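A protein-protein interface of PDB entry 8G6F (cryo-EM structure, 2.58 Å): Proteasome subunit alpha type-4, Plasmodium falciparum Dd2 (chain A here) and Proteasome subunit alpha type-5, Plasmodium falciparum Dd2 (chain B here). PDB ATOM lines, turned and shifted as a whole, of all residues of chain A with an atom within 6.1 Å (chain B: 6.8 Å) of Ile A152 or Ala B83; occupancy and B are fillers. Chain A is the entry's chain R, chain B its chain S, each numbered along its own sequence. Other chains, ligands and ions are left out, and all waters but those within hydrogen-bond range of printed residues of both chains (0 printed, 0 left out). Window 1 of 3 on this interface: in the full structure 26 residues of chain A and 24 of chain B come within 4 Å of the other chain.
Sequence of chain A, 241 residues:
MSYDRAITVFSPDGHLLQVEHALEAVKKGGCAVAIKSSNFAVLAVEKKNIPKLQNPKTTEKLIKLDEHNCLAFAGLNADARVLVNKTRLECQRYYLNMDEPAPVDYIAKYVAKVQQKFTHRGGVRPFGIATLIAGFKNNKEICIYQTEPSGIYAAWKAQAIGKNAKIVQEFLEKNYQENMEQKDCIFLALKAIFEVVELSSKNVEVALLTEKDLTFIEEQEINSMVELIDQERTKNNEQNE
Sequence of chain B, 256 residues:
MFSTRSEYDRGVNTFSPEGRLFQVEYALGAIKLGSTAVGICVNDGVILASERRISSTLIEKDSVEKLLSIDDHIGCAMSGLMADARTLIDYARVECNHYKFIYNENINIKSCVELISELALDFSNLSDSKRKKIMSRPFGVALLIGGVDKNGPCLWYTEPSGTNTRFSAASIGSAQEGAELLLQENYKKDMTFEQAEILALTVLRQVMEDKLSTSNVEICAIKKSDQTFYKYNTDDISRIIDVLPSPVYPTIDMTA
Of the 11 printed residues of chain B, 5 touch a printed residue of chain A. Printed residues of chain B that touch a printed residue of chain A: Met B82, Ala B83, Asp B84, Arg B86 and Thr B87. Of the 12 printed residues of chain A, 5 touch a printed residue of chain B. Hydrophobic or aromatic side chains of chain A that line the printed part of chain B: Ile A152 and Tyr A153.
The side-chain hydroxyl (OG1) of Thr B87 lies within hydrogen-bond range of the backbone carbonyl oxygen (O) of Ala B83, at 2.9 Å.
Printed residues of chain B within 4 Å of Gln A116: Ala B83 (3.5 Å), Asp B84 (2.8 Å) and Thr B87 (3.2 Å). Leu B81 touches none of the printed residues of chain A. Of the printed residues of chain A, Met B82 touches Ile A152 (3.98 Å). Printed residues of chain A within 4 Å of Ala B83: Gln A116 (3.5 Å), Ser A150 (3.4 Å), Gly A151 (3.9 Å) and Ile A152 (3.7 Å). Val B141 touches none of the printed residues of chain A. The nearest residue of chain B that does not touch Ile A152 is Leu B81 (5.8 Å). The nearest residue of chain A that does not touch Ala B83 is Ala A112 (6.0 Å).
The side-chain hydroxyl of Thr B87 lies within hydrogen-bond range of the side-chain amide oxygen of Gln A116 (3.2 Å). The side-chain carboxylate (OD1) of Asp B84 is in hydrogen-bond range of the side-chain amide nitrogen (NE2) of Gln A116, at 2.8 Å. The backbone carbonyl oxygen (O) of Tyr A153 lies within hydrogen-bond range of the guanidinium group (NH2) of Arg B86 (3.5 Å). The backbone carbonyl oxygen (O) of Gly A151 lies within hydrogen-bond range of the guanidinium group (NH1) of Arg B86.
Among the printed residues, pairs that only touch across the chains: Gln A116 with Ala B83 (3.5 Å), Ser A150 with Ala B83 (3.4 Å), Gly A151 with Ala B83 (3.9 Å), Ile A152 with Met B82 (3.98 Å), Ile A152 with Ala B83 (3.7 Å) and Ile A152 with Arg B86 (3.6 Å).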
ATOM      1  N   ALA A 112      18.663  36.587  14.055  1.00  0.00           N
ATOM      2  CA  ALA A 112      18.125  35.234  14.106  1.00  0.00           C
ATOM      3  C   ALA A 112      16.719  35.221  14.692  1.00  0.00           C
ATOM      4  O   ALA A 112      15.850  34.479  14.225  1.00  0.00           O
ATOM      5  CB  ALA A 112      19.057  34.343  14.921  1.00  0.00           C
ATOM      6  N   GLN A 115      14.256  36.331  12.043  1.00  0.00           N
ATOM      7  CA  GLN A 115      13.990  35.287  11.056  1.00  0.00           C
ATOM      8  C   GLN A 115      13.105  34.181  11.632  1.00  0.00           C
ATOM      9  O   GLN A 115      12.195  33.683  10.952  1.00  0.00           O
ATOM     10  CB  GLN A 115      15.311  34.735  10.532  1.00  0.00           C
ATOM     11  CG  GLN A 115      15.962  35.665   9.523  1.00  0.00           C
ATOM     12  CD  GLN A 115      17.386  35.293   9.210  1.00  0.00           C
ATOM     13  OE1 GLN A 115      18.206  35.137  10.107  1.00  0.00           O
ATOM     14  NE2 GLN A 115      17.691  35.151   7.929  1.00  0.00           N
ATOM     15  N   GLN A 116      13.339  33.792  12.887  1.00  0.00           N
ATOM     16  CA  GLN A 116      12.456  32.820  13.524  1.00  0.00           C
ATOM     17  C   GLN A 116      11.033  33.356  13.605  1.00  0.00           C
ATOM     18  O   GLN A 116      10.066  32.644  13.304  1.00  0.00           O
ATOM     19  CB  GLN A 116      12.974  32.470  14.918  1.00  0.00           C
ATOM     20  CG  GLN A 116      12.577  31.082  15.399  1.00  0.00           C
ATOM     21  CD  GLN A 116      11.140  31.003  15.881  1.00  0.00           C
ATOM     22  OE1 GLN A 116      10.580  31.982  16.368  1.00  0.00           O
ATOM     23  NE2 GLN A 116      10.538  29.831  15.749  1.00  0.00           N
ATOM     24  N   GLN A 146      26.978  33.332  11.862  1.00  0.00           N
ATOM     25  CA  GLN A 146      26.222  32.970  10.675  1.00  0.00           C
ATOM     26  C   GLN A 146      24.785  32.701  11.083  1.00  0.00           C
ATOM     27  O   GLN A 146      24.538  31.989  12.063  1.00  0.00           O
ATOM     28  CB  GLN A 146      26.814  31.744   9.984  1.00  0.00           C
ATOM     29  CG  GLN A 146      26.395  31.596   8.538  1.00  0.00           C
ATOM     30  CD  GLN A 146      25.615  30.328   8.283  1.00  0.00           C
ATOM     31  OE1 GLN A 146      26.018  29.245   8.698  1.00  0.00           O
ATOM     32  NE2 GLN A 146      24.492  30.456   7.593  1.00  0.00           N
ATOM     33  N   THR A 147      23.851  33.283  10.337  1.00  0.00           N
ATOM     34  CA  THR A 147      22.424  33.121  10.561  1.00  0.00           C
ATOM     35  C   THR A 147      21.779  32.581   9.295  1.00  0.00           C
ATOM     36  O   THR A 147      22.161  32.960   8.186  1.00  0.00           O
ATOM     37  CB  THR A 147      21.764  34.449  10.952  1.00  0.00           C
ATOM     38  OG1 THR A 147      22.639  35.194  11.805  1.00  0.00           O
ATOM     39  CG2 THR A 147      20.464  34.194  11.676  1.00  0.00           C
ATOM     40  N   GLU A 148      20.795  31.702   9.472  1.00  0.00           N
ATOM     41  CA  GLU A 148      20.142  31.013   8.368  1.00  0.00           C
ATOM     42  C   GLU A 148      18.666  31.381   8.302  1.00  0.00           C
ATOM     43  O   GLU A 148      18.132  31.976   9.245  1.00  0.00           O
ATOM     44  CB  GLU A 148      20.298  29.501   8.523  1.00  0.00           C
ATOM     45  CG  GLU A 148      21.625  28.962   8.036  1.00  0.00           C
ATOM     46  CD  GLU A 148      21.631  27.452   7.923  1.00  0.00           C
ATOM     47  OE1 GLU A 148      20.636  26.821   8.335  1.00  0.00           O
ATOM     48  OE2 GLU A 148      22.626  26.896   7.414  1.00  0.00           O
ATOM     49  N   PRO A 149      17.973  31.046   7.211  1.00  0.00           N
ATOM     50  CA  PRO A 149      16.541  31.379   7.126  1.00  0.00           C
ATOM     51  C   PRO A 149      15.706  30.783   8.244  1.00  0.00           C
ATOM     52  O   PRO A 149      14.720  31.400   8.660  1.00  0.00           O
ATOM     53  CB  PRO A 149      16.134  30.815   5.758  1.00  0.00           C
ATOM     54  CG  PRO A 149      17.394  30.742   4.982  1.00  0.00           C
ATOM     55  CD  PRO A 149      18.473  30.441   5.967  1.00  0.00           C
ATOM     56  N   SER A 150      16.063  29.597   8.739  1.00  0.00           N
ATOM     57  CA  SER A 150      15.315  28.986   9.829  1.00  0.00           C
ATOM     58  C   SER A 150      15.409  29.789  11.117  1.00  0.00           C
ATOM     59  O   SER A 150      14.565  29.615  12.002  1.00  0.00           O
ATOM     60  CB  SER A 150      15.821  27.568  10.079  1.00  0.00           C
ATOM     61  OG  SER A 150      17.230  27.512   9.989  1.00  0.00           O
ATOM     62  N   GLY A 151      16.403  30.659  11.240  1.00  0.00           N
ATOM     63  CA  GLY A 151      16.624  31.411  12.452  1.00  0.00           C
ATOM     64  C   GLY A 151      17.671  30.838  13.376  1.00  0.00           C
ATOM     65  O   GLY A 151      17.828  31.346  14.489  1.00  0.00           O
ATOM     66  N   ILE A 152      18.384  29.798  12.963  1.00  0.00           N
ATOM     67  CA  ILE A 152      19.450  29.225  13.771  1.00  0.00           C
ATOM     68  C   ILE A 152      20.740  29.974  13.474  1.00  0.00           C
ATOM     69  O   ILE A 152      21.092  30.190  12.309  1.00  0.00           O
ATOM     70  CB  ILE A 152      19.605  27.716  13.509  1.00  0.00           C
ATOM     71  CG1 ILE A 152      19.846  27.429  12.028  1.00  0.00           C
ATOM     72  CG2 ILE A 152      18.374  26.973  13.982  1.00  0.00           C
ATOM     73  CD1 ILE A 152      20.407  26.053  11.761  1.00  0.00           C
ATOM     74  N   TYR A 153      21.435  30.385  14.528  1.00  0.00           N
ATOM     75  CA  TYR A 153      22.677  31.127  14.410  1.00  0.00           C
ATOM     76  C   TYR A 153      23.799  30.360  15.094  1.00  0.00           C
ATOM     77  O   TYR A 153      23.570  29.551  15.994  1.00  0.00           O
ATOM     78  CB  TYR A 153      22.551  32.525  15.022  1.00  0.00           C
ATOM     79  CG  TYR A 153      22.345  32.520  16.516  1.00  0.00           C
ATOM     80  CD1 TYR A 153      23.424  32.545  17.383  1.00  0.00           C
ATOM     81  CD2 TYR A 153      21.071  32.493  17.059  1.00  0.00           C
ATOM     82  CE1 TYR A 153      23.241  32.535  18.745  1.00  0.00           C
ATOM     83  CE2 TYR A 153      20.878  32.485  18.420  1.00  0.00           C
ATOM     84  CZ  TYR A 153      21.968  32.507  19.259  1.00  0.00           C
ATOM     85  OH  TYR A 153      21.783  32.502  20.621  1.00  0.00           O
ATOM     86  N   ALA A 154      25.022  30.619  14.644  1.00  0.00           N
ATOM     87  CA  ALA A 154      26.184  29.995  15.264  1.00  0.00           C
ATOM     88  C   ALA A 154      27.417  30.833  14.979  1.00  0.00           C
ATOM     89  O   ALA A 154      27.543  31.422  13.907  1.00  0.00           O
ATOM     90  CB  ALA A 154      26.385  28.565  14.761  1.00  0.00           C
ATOM     91  N   GLY B  80      14.837  18.952  18.836  1.00  0.00           N
ATOM     92  CA  GLY B  80      13.903  19.343  17.801  1.00  0.00           C
ATOM     93  C   GLY B  80      14.442  20.468  16.946  1.00  0.00           C
ATOM     94  O   GLY B  80      15.592  20.415  16.503  1.00  0.00           O
ATOM     95  N   LEU B  81      13.628  21.491  16.707  1.00  0.00           N
ATOM     96  CA  LEU B  81      14.060  22.670  15.969  1.00  0.00           C
ATOM     97  C   LEU B  81      14.732  23.633  16.937  1.00  0.00           C
ATOM     98  O   LEU B  81      14.113  24.074  17.911  1.00  0.00           O
ATOM     99  CB  LEU B  81      12.878  23.339  15.273  1.00  0.00           C
ATOM    100  CG  LEU B  81      12.124  22.495  14.245  1.00  0.00           C
ATOM    101  CD1 LEU B  81      10.963  23.284  13.679  1.00  0.00           C
ATOM    102  CD2 LEU B  81      13.041  22.036  13.132  1.00  0.00           C
ATOM    103  N   MET B  82      15.993  23.966  16.665  1.00  0.00           N
ATOM    104  CA  MET B  82      16.777  24.736  17.624  1.00  0.00           C
ATOM    105  C   MET B  82      16.294  26.176  17.723  1.00  0.00           C
ATOM    106  O   MET B  82      16.341  26.774  18.801  1.00  0.00           O
ATOM    107  CB  MET B  82      18.255  24.699  17.244  1.00  0.00           C
ATOM    108  CG  MET B  82      19.028  23.515  17.811  1.00  0.00           C
ATOM    109  SD  MET B  82      18.795  23.232  19.578  1.00  0.00           S
ATOM    110  CE  MET B  82      17.650  21.855  19.540  1.00  0.00           C
ATOM    111  N   ALA B  83      15.842  26.762  16.614  1.00  0.00           N
ATOM    112  CA  ALA B  83      15.331  28.127  16.678  1.00  0.00           C
ATOM    113  C   ALA B  83      14.080  28.202  17.544  1.00  0.00           C
ATOM    114  O   ALA B  83      13.949  29.096  18.392  1.00  0.00           O
ATOM    115  CB  ALA B  83      15.050  28.641  15.271  1.00  0.00           C
ATOM    116  N   ASP B  84      13.178  27.236  17.359  1.00  0.00           N
ATOM    117  CA  ASP B  84      11.949  27.192  18.194  1.00  0.00           C
ATOM    118  C   ASP B  84      12.346  26.931  19.652  1.00  0.00           C
ATOM    119  O   ASP B  84      11.718  27.531  20.547  1.00  0.00           O
ATOM    120  CB  ASP B  84      10.951  26.159  17.663  1.00  0.00           C
ATOM    121  CG  ASP B  84       9.827  26.778  16.853  1.00  0.00           C
ATOM    122  OD1 ASP B  84       9.342  27.853  17.254  1.00  0.00           O
ATOM    123  OD2 ASP B  84       9.451  26.184  15.825  1.00  0.00           O
ATOM    124  N   ALA B  85      13.353  26.079  19.877  1.00  0.00           N
ATOM    125  CA  ALA B  85      13.792  25.808  21.240  1.00  0.00           C
ATOM    126  C   ALA B  85      14.328  27.069  21.902  1.00  0.00           C
ATOM    127  O   ALA B  85      14.036  27.334  23.071  1.00  0.00           O
ATOM    128  CB  ALA B  85      14.853  24.711  21.239  1.00  0.00           C
ATOM    129  N   ARG B  86      15.120  27.852  21.177  1.00  0.00           N
ATOM    130  CA  ARG B  86      15.653  29.084  21.745  1.00  0.00           C
ATOM    131  C   ARG B  86      14.539  30.084  22.026  1.00  0.00           C
ATOM    132  O   ARG B  86      14.564  30.775  23.049  1.00  0.00           O
ATOM    133  CB  ARG B  86      16.700  29.680  20.807  1.00  0.00           C
ATOM    134  CG  ARG B  86      18.021  28.934  20.839  1.00  0.00           C
ATOM    135  CD  ARG B  86      19.151  29.765  20.273  1.00  0.00           C
ATOM    136  NE  ARG B  86      19.911  29.042  19.258  1.00  0.00           N
ATOM    137  CZ  ARG B  86      19.700  29.124  17.950  1.00  0.00           C
ATOM    138  NH1 ARG B  86      18.734  29.878  17.448  1.00  0.00           N
ATOM    139  NH2 ARG B  86      20.477  28.432  17.124  1.00  0.00           N
ATOM    140  N   THR B  87      13.548  30.166  21.139  1.00  0.00           N
ATOM    141  CA  THR B  87      12.399  31.031  21.395  1.00  0.00           C
ATOM    142  C   THR B  87      11.665  30.607  22.663  1.00  0.00           C
ATOM    143  O   THR B  87      11.323  31.440  23.514  1.00  0.00           O
ATOM    144  CB  THR B  87      11.460  31.003  20.189  1.00  0.00           C
ATOM    145  OG1 THR B  87      12.206  31.290  19.002  1.00  0.00           O
ATOM    146  CG2 THR B  87      10.346  32.016  20.340  1.00  0.00           C
ATOM    147  N   LEU B  88      11.430  29.302  22.812  1.00  0.00           N
ATOM    148  CA  LEU B  88      10.738  28.796  23.993  1.00  0.00           C
ATOM    149  C   LEU B  88      11.535  29.065  25.260  1.00  0.00           C
ATOM    150  O   LEU B  88      10.970  29.449  26.290  1.00  0.00           O
ATOM    151  CB  LEU B  88      10.483  27.296  23.847  1.00  0.00           C
ATOM    152  CG  LEU B  88       9.068  26.837  23.508  1.00  0.00           C
ATOM    153  CD1 LEU B  88       9.045  25.337  23.353  1.00  0.00           C
ATOM    154  CD2 LEU B  88       8.082  27.268  24.567  1.00  0.00           C
ATOM    155  N   PHE B 139       5.436  24.270  18.091  1.00  0.00           N
ATOM    156  CA  PHE B 139       6.857  24.574  18.181  1.00  0.00           C
ATOM    157  C   PHE B 139       7.745  23.448  17.672  1.00  0.00           C
ATOM    158  O   PHE B 139       8.833  23.718  17.155  1.00  0.00           O
ATOM    159  CB  PHE B 139       7.234  24.900  19.626  1.00  0.00           C
ATOM    160  CG  PHE B 139       7.072  26.344  19.979  1.00  0.00           C
ATOM    161  CD1 PHE B 139       5.831  26.857  20.305  1.00  0.00           C
ATOM    162  CD2 PHE B 139       8.161  27.193  19.981  1.00  0.00           C
ATOM    163  CE1 PHE B 139       5.682  28.188  20.630  1.00  0.00           C
ATOM    164  CE2 PHE B 139       8.016  28.524  20.305  1.00  0.00           C
ATOM    165  CZ  PHE B 139       6.776  29.021  20.631  1.00  0.00           C
ATOM    166  N   VAL B 141       9.310  21.148  19.478  1.00  0.00           N
ATOM    167  CA  VAL B 141      10.440  21.190  20.395  1.00  0.00           C
ATOM    168  C   VAL B 141      10.125  20.299  21.585  1.00  0.00           C
ATOM    169  O   VAL B 141       9.006  20.316  22.106  1.00  0.00           O
ATOM    170  CB  VAL B 141      10.728  22.632  20.858  1.00  0.00           C
ATOM    171  CG1 VAL B 141      11.723  22.637  22.000  1.00  0.00           C
ATOM    172  CG2 VAL B 141      11.228  23.461  19.703  1.00  0.00           C
